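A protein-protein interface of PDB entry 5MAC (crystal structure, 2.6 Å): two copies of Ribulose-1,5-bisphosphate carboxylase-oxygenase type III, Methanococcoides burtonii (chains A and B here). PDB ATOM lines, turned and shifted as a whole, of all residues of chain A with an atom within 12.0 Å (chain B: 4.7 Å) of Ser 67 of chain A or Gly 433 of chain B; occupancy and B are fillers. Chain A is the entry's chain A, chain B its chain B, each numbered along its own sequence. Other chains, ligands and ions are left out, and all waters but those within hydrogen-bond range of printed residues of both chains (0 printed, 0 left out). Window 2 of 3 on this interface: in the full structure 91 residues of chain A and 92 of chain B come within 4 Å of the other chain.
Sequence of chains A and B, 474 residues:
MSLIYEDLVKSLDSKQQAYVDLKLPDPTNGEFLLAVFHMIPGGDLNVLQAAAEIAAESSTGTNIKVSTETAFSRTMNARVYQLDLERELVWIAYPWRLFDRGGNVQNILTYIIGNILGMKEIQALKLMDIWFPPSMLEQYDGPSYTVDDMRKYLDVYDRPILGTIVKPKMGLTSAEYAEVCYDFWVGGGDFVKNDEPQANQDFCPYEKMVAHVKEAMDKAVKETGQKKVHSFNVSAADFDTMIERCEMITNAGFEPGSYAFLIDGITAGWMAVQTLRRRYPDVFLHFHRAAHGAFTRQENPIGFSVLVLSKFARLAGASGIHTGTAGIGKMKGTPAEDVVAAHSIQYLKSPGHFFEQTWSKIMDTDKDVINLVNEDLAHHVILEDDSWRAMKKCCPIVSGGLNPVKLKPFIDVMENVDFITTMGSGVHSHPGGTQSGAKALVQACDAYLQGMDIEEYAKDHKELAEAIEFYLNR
A ring nitrogen (ND1) of His 428 of chain B lies within hydrogen-bond range of the side-chain hydroxyl (OG1) of Thr 434 of chain B (2.9 Å).
Among the printed residues, pairs that only touch across the chains: Ile 64 of chain A with Ser 429 of chain B, Lys 65 of chain A with Ser 429 of chain B, Val 66 of chain A with His 428 of chain B, Val 66 of chain A with Ser 429 of chain B, Ser 67 of chain A with Gly 433 of chain B, Thr 68 of chain A with His 428 of chain B and Thr 68 of chain A with Thr 434 of chain B.
Of the 11 printed residues of chain B, 4 touch a printed residue of chain A.
Hydrophobic or aromatic side chains of chain B that line the printed part of chain A: His 428.
Of the 18 printed residues of chain A, 5 touch a printed residue of chain B.
Hydrophobic or aromatic side chains of chain A that line the printed part of chain B: Ile 64 and Val 66.
Among the printed residues, 8 pairs touch across the chains.
The side-chain hydroxyl (OG) of Ser 67 of chain A is in hydrogen-bond range of the backbone carbonyl oxygen (O) of His 428 of chain B.
No position is printed for both chains.
Of the 8 pairs that touch across the chains among the printed residues, none has its exchanged pair printed and touching as well.
Ser 67 of chain A touches just these residues of chain B: His 428 and Gly 433.
Of chain A, only Ser 67 comes within 4 Å of Gly 433 of chain B.
No residue of chain A comes within 4 Å of Val 427 of chain B.
Of chain A, only Val 66, Ser 67 and Thr 68 come within 4 Å of His 428 of chain B.
Of chain A, only Ile 64 (3.5 Å), Lys 65 (3.2 Å) and Val 66 (3.97 Å) come within 4 Å of Ser 429 of chain B.
No residue of chain A comes within 4 Å of His 430 of chain B.
No residue of chain A comes within 4 Å of Gly 432 of chain B.
No residue of chain A comes within 4 Å of Ser 436 of chain B.
Of the printed residues of chain B, Val 66 of chain A touches His 428 and Ser 429.
Of the printed residues of chain B, Ile 64 of chain A touches Ser 429 (3.5 Å).
Of the printed residues of chain B, Thr 68 of chain A touches His 428 and Thr 434.
Of the printed residues of chain B, Lys 65 of chain A touches Ser 429 (3.2 Å).
The nearest residue of chain B that does not touch Ser 67 of chain A is Thr 434 of chain B (4.2 Å).
The nearest residue of chain A that does not touch Gly 433 of chain B is Thr 68 of chain A (6.5 Å).
The nearest printed residue of chain B that does not touch Lys 65 of chain A is His 428 of chain B (5.1 Å).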
ATOM      1  N   SER A  14      15.995   2.639   8.769  1.00  0.00           N
ATOM      2  CA  SER A  14      16.445   4.021   8.594  1.00  0.00           C
ATOM      3  C   SER A  14      16.500   4.364   7.069  1.00  0.00           C
ATOM      4  O   SER A  14      16.340   5.532   6.674  1.00  0.00           O
ATOM      5  CB  SER A  14      17.800   4.239   9.262  1.00  0.00           C
ATOM      6  OG  SER A  14      18.746   3.246   8.888  1.00  0.00           O
ATOM      7  N   LYS A  15      16.698   3.328   6.224  1.00  0.00           N
ATOM      8  CA  LYS A  15      16.720   3.468   4.778  1.00  0.00           C
ATOM      9  C   LYS A  15      15.286   3.635   4.259  1.00  0.00           C
ATOM     10  O   LYS A  15      14.987   4.627   3.599  1.00  0.00           O
ATOM     11  CB  LYS A  15      17.383   2.250   4.138  1.00  0.00           C
ATOM     12  CG  LYS A  15      17.834   2.493   2.701  1.00  0.00           C
ATOM     13  CD  LYS A  15      17.748   1.256   1.866  1.00  0.00           C
ATOM     14  CE  LYS A  15      16.350   1.021   1.351  1.00  0.00           C
ATOM     15  NZ  LYS A  15      16.128  -0.402   1.084  1.00  0.00           N
ATOM     16  N   TYR A  19      12.269   6.993   2.258  1.00  0.00           N
ATOM     17  CA  TYR A  19      11.415   6.940   1.066  1.00  0.00           C
ATOM     18  C   TYR A  19       9.936   6.868   1.415  1.00  0.00           C
ATOM     19  O   TYR A  19       9.143   6.287   0.675  1.00  0.00           O
ATOM     20  CB  TYR A  19      11.835   5.775   0.174  1.00  0.00           C
ATOM     21  CG  TYR A  19      13.267   5.908  -0.278  1.00  0.00           C
ATOM     22  CD1 TYR A  19      13.586   6.551  -1.464  1.00  0.00           C
ATOM     23  CD2 TYR A  19      14.310   5.454   0.513  1.00  0.00           C
ATOM     24  CE1 TYR A  19      14.904   6.745  -1.845  1.00  0.00           C
ATOM     25  CE2 TYR A  19      15.627   5.550   0.092  1.00  0.00           C
ATOM     26  CZ  TYR A  19      15.926   6.222  -1.074  1.00  0.00           C
ATOM     27  OH  TYR A  19      17.242   6.352  -1.438  1.00  0.00           O
ATOM     28  N   THR A  60      16.591   7.044  -6.005  1.00  0.00           N
ATOM     29  CA  THR A  60      17.981   7.217  -5.613  1.00  0.00           C
ATOM     30  C   THR A  60      18.619   6.074  -4.796  1.00  0.00           C
ATOM     31  O   THR A  60      19.816   6.150  -4.484  1.00  0.00           O
ATOM     32  CB  THR A  60      17.998   8.460  -4.732  1.00  0.00           C
ATOM     33  OG1 THR A  60      17.122   8.194  -3.652  1.00  0.00           O
ATOM     34  CG2 THR A  60      17.485   9.726  -5.438  1.00  0.00           C
ATOM     35  N   GLY A  61      17.834   5.065  -4.417  1.00  0.00           N
ATOM     36  CA  GLY A  61      18.286   4.032  -3.494  1.00  0.00           C
ATOM     37  C   GLY A  61      18.674   2.674  -4.011  1.00  0.00           C
ATOM     38  O   GLY A  61      18.675   2.408  -5.212  1.00  0.00           O
ATOM     39  N   THR A  62      19.033   1.804  -3.048  1.00  0.00           N
ATOM     40  CA  THR A  62      19.390   0.403  -3.298  1.00  0.00           C
ATOM     41  C   THR A  62      18.979  -0.430  -2.089  1.00  0.00           C
ATOM     42  O   THR A  62      18.438   0.145  -1.163  1.00  0.00           O
ATOM     43  CB  THR A  62      20.856   0.313  -3.735  1.00  0.00           C
ATOM     44  OG1 THR A  62      21.139  -1.037  -4.181  1.00  0.00           O
ATOM     45  CG2 THR A  62      21.832   0.835  -2.657  1.00  0.00           C
ATOM     46  N   ASN A  63      19.173  -1.771  -2.097  1.00  0.00           N
ATOM     47  CA  ASN A  63      18.678  -2.620  -0.991  1.00  0.00           C
ATOM     48  C   ASN A  63      19.376  -2.375   0.380  1.00  0.00           C
ATOM     49  O   ASN A  63      18.802  -2.771   1.404  1.00  0.00           O
ATOM     50  CB  ASN A  63      18.654  -4.123  -1.346  1.00  0.00           C
ATOM     51  CG  ASN A  63      19.968  -4.738  -1.717  1.00  0.00           C
ATOM     52  OD1 ASN A  63      20.710  -4.191  -2.532  1.00  0.00           O
ATOM     53  ND2 ASN A  63      20.235  -5.944  -1.220  1.00  0.00           N
ATOM     54  N   ILE A  64      20.545  -1.703   0.413  1.00  0.00           N
ATOM     55  CA  ILE A  64      21.225  -1.327   1.654  1.00  0.00           C
ATOM     56  C   ILE A  64      21.642   0.154   1.563  1.00  0.00           C
ATOM     57  O   ILE A  64      22.134   0.578   0.518  1.00  0.00           O
ATOM     58  CB  ILE A  64      22.473  -2.225   1.925  1.00  0.00           C
ATOM     59  CG1 ILE A  64      22.119  -3.718   1.875  1.00  0.00           C
ATOM     60  CG2 ILE A  64      23.127  -1.900   3.280  1.00  0.00           C
ATOM     61  CD1 ILE A  64      23.309  -4.628   1.892  1.00  0.00           C
ATOM     62  N   LYS A  65      21.510   0.928   2.671  1.00  0.00           N
ATOM     63  CA  LYS A  65      21.977   2.323   2.673  1.00  0.00           C
ATOM     64  C   LYS A  65      23.509   2.349   2.392  1.00  0.00           C
ATOM     65  O   LYS A  65      24.243   1.496   2.895  1.00  0.00           O
ATOM     66  CB  LYS A  65      21.570   3.096   3.964  1.00  0.00           C
ATOM     67  CG  LYS A  65      22.280   2.710   5.253  1.00  0.00           C
ATOM     68  CD  LYS A  65      21.611   3.354   6.491  1.00  0.00           C
ATOM     69  CE  LYS A  65      21.782   4.858   6.555  1.00  0.00           C
ATOM     70  NZ  LYS A  65      21.348   5.419   7.868  1.00  0.00           N
ATOM     71  N   VAL A  66      23.959   3.294   1.535  1.00  0.00           N
ATOM     72  CA  VAL A  66      25.354   3.358   1.093  1.00  0.00           C
ATOM     73  C   VAL A  66      26.150   4.487   1.744  1.00  0.00           C
ATOM     74  O   VAL A  66      25.602   5.522   2.099  1.00  0.00           O
ATOM     75  CB  VAL A  66      25.481   3.400  -0.458  1.00  0.00           C
ATOM     76  CG1 VAL A  66      25.059   2.070  -1.070  1.00  0.00           C
ATOM     77  CG2 VAL A  66      24.686   4.539  -1.072  1.00  0.00           C
ATOM     78  N   SER A  67      27.458   4.268   1.878  1.00  0.00           N
ATOM     79  CA  SER A  67      28.412   5.244   2.423  1.00  0.00           C
ATOM     80  C   SER A  67      28.558   6.477   1.493  1.00  0.00           C
ATOM     81  O   SER A  67      28.892   7.566   1.955  1.00  0.00           O
ATOM     82  CB  SER A  67      29.785   4.589   2.600  1.00  0.00           C
ATOM     83  OG  SER A  67      30.355   4.171   1.366  1.00  0.00           O
ATOM     84  N   THR A  68      28.326   6.282   0.186  1.00  0.00           N
ATOM     85  CA  THR A  68      28.446   7.312  -0.853  1.00  0.00           C
ATOM     86  C   THR A  68      27.267   8.330  -0.913  1.00  0.00           C
ATOM     87  O   THR A  68      27.342   9.296  -1.664  1.00  0.00           O
ATOM     88  CB  THR A  68      28.630   6.604  -2.192  1.00  0.00           C
ATOM     89  OG1 THR A  68      27.588   5.640  -2.329  1.00  0.00           O
ATOM     90  CG2 THR A  68      29.987   5.890  -2.287  1.00  0.00           C
ATOM     91  N   GLU A  69      26.208   8.109  -0.133  1.00  0.00           N
ATOM     92  CA  GLU A  69      25.016   8.949  -0.048  1.00  0.00           C
ATOM     93  C   GLU A  69      25.320  10.331   0.514  1.00  0.00           C
ATOM     94  O   GLU A  69      26.090  10.464   1.455  1.00  0.00           O
ATOM     95  CB  GLU A  69      23.999   8.227   0.852  1.00  0.00           C
ATOM     96  CG  GLU A  69      22.753   8.981   1.291  1.00  0.00           C
ATOM     97  CD  GLU A  69      21.955   8.205   2.327  1.00  0.00           C
ATOM     98  OE1 GLU A  69      22.106   6.963   2.407  1.00  0.00           O
ATOM     99  OE2 GLU A  69      21.214   8.854   3.100  1.00  0.00           O
ATOM    100  N   THR A  70      24.652  11.349  -0.031  1.00  0.00           N
ATOM    101  CA  THR A  70      24.803  12.756   0.348  1.00  0.00           C
ATOM    102  C   THR A  70      23.460  13.354   0.802  1.00  0.00           C
ATOM    103  O   THR A  70      22.401  12.798   0.503  1.00  0.00           O
ATOM    104  CB  THR A  70      25.357  13.566  -0.858  1.00  0.00           C
ATOM    105  OG1 THR A  70      24.383  13.596  -1.913  1.00  0.00           O
ATOM    106  CG2 THR A  70      26.662  12.994  -1.390  1.00  0.00           C
ATOM    107  N   ALA A  71      23.508  14.513   1.486  1.00  0.00           N
ATOM    108  CA  ALA A  71      22.284  15.207   1.890  1.00  0.00           C
ATOM    109  C   ALA A  71      21.511  15.685   0.672  1.00  0.00           C
ATOM    110  O   ALA A  71      20.288  15.676   0.689  1.00  0.00           O
ATOM    111  CB  ALA A  71      22.621  16.387   2.773  1.00  0.00           C
ATOM    112  N   PHE A  72      22.238  16.083  -0.391  1.00  0.00           N
ATOM    113  CA  PHE A  72      21.672  16.592  -1.635  1.00  0.00           C
ATOM    114  C   PHE A  72      20.960  15.485  -2.371  1.00  0.00           C
ATOM    115  O   PHE A  72      19.931  15.732  -2.987  1.00  0.00           O
ATOM    116  CB  PHE A  72      22.760  17.240  -2.506  1.00  0.00           C
ATOM    117  CG  PHE A  72      22.236  17.861  -3.786  1.00  0.00           C
ATOM    118  CD1 PHE A  72      21.507  19.039  -3.760  1.00  0.00           C
ATOM    119  CD2 PHE A  72      22.419  17.230  -5.009  1.00  0.00           C
ATOM    120  CE1 PHE A  72      20.954  19.561  -4.932  1.00  0.00           C
ATOM    121  CE2 PHE A  72      21.874  17.760  -6.181  1.00  0.00           C
ATOM    122  CZ  PHE A  72      21.145  18.919  -6.137  1.00  0.00           C
ATOM    123  N   SER A  73      21.505  14.263  -2.316  1.00  0.00           N
ATOM    124  CA  SER A  73      20.886  13.093  -2.956  1.00  0.00           C
ATOM    125  C   SER A  73      19.551  12.726  -2.296  1.00  0.00           C
ATOM    126  O   SER A  73      18.634  12.320  -3.002  1.00  0.00           O
ATOM    127  CB  SER A  73      21.843  11.897  -2.964  1.00  0.00           C
ATOM    128  OG  SER A  73      22.133  11.329  -1.697  1.00  0.00           O
ATOM    129  N   ARG A  74      19.432  12.933  -0.952  1.00  0.00           N
ATOM    130  CA  ARG A  74      18.216  12.643  -0.200  1.00  0.00           C
ATOM    131  C   ARG A  74      17.061  13.556  -0.617  1.00  0.00           C
ATOM    132  O   ARG A  74      15.907  13.135  -0.595  1.00  0.00           O
ATOM    133  CB  ARG A  74      18.456  12.760   1.310  1.00  0.00           C
ATOM    134  CG  ARG A  74      19.252  11.618   1.923  1.00  0.00           C
ATOM    135  CD  ARG A  74      19.106  11.589   3.444  1.00  0.00           C
ATOM    136  NE  ARG A  74      19.909  12.606   4.139  1.00  0.00           N
ATOM    137  CZ  ARG A  74      21.220  12.536   4.384  1.00  0.00           C
ATOM    138  NH1 ARG A  74      21.934  11.499   3.953  1.00  0.00           N
ATOM    139  NH2 ARG A  74      21.832  13.517   5.040  1.00  0.00           N
ATOM    140  N   VAL B 427      28.988  -3.277  -2.397  1.00  0.00           N
ATOM    141  CA  VAL B 427      30.322  -2.659  -2.337  1.00  0.00           C
ATOM    142  C   VAL B 427      30.294  -1.333  -1.564  1.00  0.00           C
ATOM    143  O   VAL B 427      31.098  -1.158  -0.657  1.00  0.00           O
ATOM    144  CB  VAL B 427      30.892  -2.482  -3.770  1.00  0.00           C
ATOM    145  CG1 VAL B 427      32.029  -1.472  -3.808  1.00  0.00           C
ATOM    146  CG2 VAL B 427      31.349  -3.816  -4.342  1.00  0.00           C
ATOM    147  N   HIS B 428      29.368  -0.414  -1.901  1.00  0.00           N
ATOM    148  CA  HIS B 428      29.341   0.940  -1.299  1.00  0.00           C
ATOM    149  C   HIS B 428      28.698   1.002   0.077  1.00  0.00           C
ATOM    150  O   HIS B 428      28.829   2.035   0.733  1.00  0.00           O
ATOM    151  CB  HIS B 428      28.677   1.988  -2.245  1.00  0.00           C
ATOM    152  CG  HIS B 428      29.108   1.880  -3.674  1.00  0.00           C
ATOM    153  ND1 HIS B 428      30.415   2.125  -4.053  1.00  0.00           N
ATOM    154  CD2 HIS B 428      28.399   1.496  -4.759  1.00  0.00           C
ATOM    155  CE1 HIS B 428      30.462   1.880  -5.347  1.00  0.00           C
ATOM    156  NE2 HIS B 428      29.263   1.535  -5.823  1.00  0.00           N
ATOM    157  N   SER B 429      28.008  -0.059   0.513  1.00  0.00           N
ATOM    158  CA  SER B 429      27.434  -0.134   1.861  1.00  0.00           C
ATOM    159  C   SER B 429      28.420  -0.773   2.851  1.00  0.00           C
ATOM    160  O   SER B 429      28.119  -0.870   4.042  1.00  0.00           O
ATOM    161  CB  SER B 429      26.129  -0.930   1.851  1.00  0.00           C
ATOM    162  OG  SER B 429      26.355  -2.328   1.814  1.00  0.00           O
ATOM    163  N   HIS B 430      29.577  -1.218   2.372  1.00  0.00           N
ATOM    164  CA  HIS B 430      30.564  -1.856   3.213  1.00  0.00           C
ATOM    165  C   HIS B 430      30.969  -0.907   4.320  1.00  0.00           C
ATOM    166  O   HIS B 430      31.220   0.264   4.032  1.00  0.00           O
ATOM    167  CB  HIS B 430      31.815  -2.230   2.376  1.00  0.00           C
ATOM    168  CG  HIS B 430      32.852  -3.035   3.114  1.00  0.00           C
ATOM    169  ND1 HIS B 430      33.729  -2.448   4.020  1.00  0.00           N
ATOM    170  CD2 HIS B 430      33.138  -4.350   3.028  1.00  0.00           C
ATOM    171  CE1 HIS B 430      34.521  -3.421   4.437  1.00  0.00           C
ATOM    172  NE2 HIS B 430      34.210  -4.579   3.858  1.00  0.00           N
ATOM    173  N   PRO B 431      31.130  -1.421   5.562  1.00  0.00           N
ATOM    174  CA  PRO B 431      31.582  -0.569   6.690  1.00  0.00           C
ATOM    175  C   PRO B 431      32.726   0.439   6.422  1.00  0.00           C
ATOM    176  O   PRO B 431      32.694   1.515   7.007  1.00  0.00           O
ATOM    177  CB  PRO B 431      32.005  -1.598   7.746  1.00  0.00           C
ATOM    178  CG  PRO B 431      31.195  -2.796   7.459  1.00  0.00           C
ATOM    179  CD  PRO B 431      30.868  -2.806   6.010  1.00  0.00           C
ATOM    180  N   GLY B 432      33.701   0.092   5.580  1.00  0.00           N
ATOM    181  CA  GLY B 432      34.814   0.977   5.240  1.00  0.00           C
ATOM    182  C   GLY B 432      34.687   1.734   3.920  1.00  0.00           C
ATOM    183  O   GLY B 432      35.654   2.372   3.468  1.00  0.00           O
ATOM    184  N   GLY B 433      33.509   1.633   3.283  1.00  0.00           N
ATOM    185  CA  GLY B 433      33.209   2.293   2.022  1.00  0.00           C
ATOM    186  C   GLY B 433      33.674   1.559   0.790  1.00  0.00           C
ATOM    187  O   GLY B 433      34.079   0.407   0.879  1.00  0.00           O
ATOM    188  N   THR B 434      33.607   2.237  -0.373  1.00  0.00           N
ATOM    189  CA  THR B 434      33.887   1.671  -1.700  1.00  0.00           C
ATOM    190  C   THR B 434      35.254   0.969  -1.854  1.00  0.00           C
ATOM    191  O   THR B 434      35.300  -0.082  -2.484  1.00  0.00           O
ATOM    192  CB  THR B 434      33.703   2.739  -2.800  1.00  0.00           C
ATOM    193  OG1 THR B 434      32.487   3.456  -2.599  1.00  0.00           O
ATOM    194  CG2 THR B 434      33.675   2.144  -4.182  1.00  0.00           C
ATOM    195  N   GLN B 435      36.341   1.535  -1.317  1.00  0.00           N
ATOM    196  CA  GLN B 435      37.680   0.943  -1.452  1.00  0.00           C
ATOM    197  C   GLN B 435      37.785  -0.382  -0.713  1.00  0.00           C
ATOM    198  O   GLN B 435      38.310  -1.365  -1.247  1.00  0.00           O
ATOM    199  CB  GLN B 435      38.768   1.912  -0.965  1.00  0.00           C
ATOM    200  CG  GLN B 435      39.101   3.037  -1.965  1.00  0.00           C
ATOM    201  CD  GLN B 435      40.333   3.850  -1.611  1.00  0.00           C
ATOM    202  OE1 GLN B 435      41.260   3.384  -0.942  1.00  0.00           O
ATOM    203  NE2 GLN B 435      40.413   5.070  -2.114  1.00  0.00           N
ATOM    204  N   SER B 436      37.284  -0.403   0.525  1.00  0.00           N
ATOM    205  CA  SER B 436      37.233  -1.617   1.331  1.00  0.00           C
ATOM    206  C   SER B 436      36.188  -2.558   0.748  1.00  0.00           C
ATOM    207  O   SER B 436      36.418  -3.762   0.654  1.00  0.00           O
ATOM    208  CB  SER B 436      36.948  -1.283   2.791  1.00  0.00           C
ATOM    209  OG  SER B 436      38.052  -0.586   3.340  1.00  0.00           O
ATOM    210  N   GLY B 437      35.071  -1.995   0.320  1.00  0.00           N
ATOM    211  CA  GLY B 437      34.014  -2.713  -0.375  1.00  0.00           C
ATOM    212  C   GLY B 437      34.490  -3.487  -1.586  1.00  0.00           C
ATOM    213  O   GLY B 437      34.043  -4.611  -1.808  1.00  0.00           O
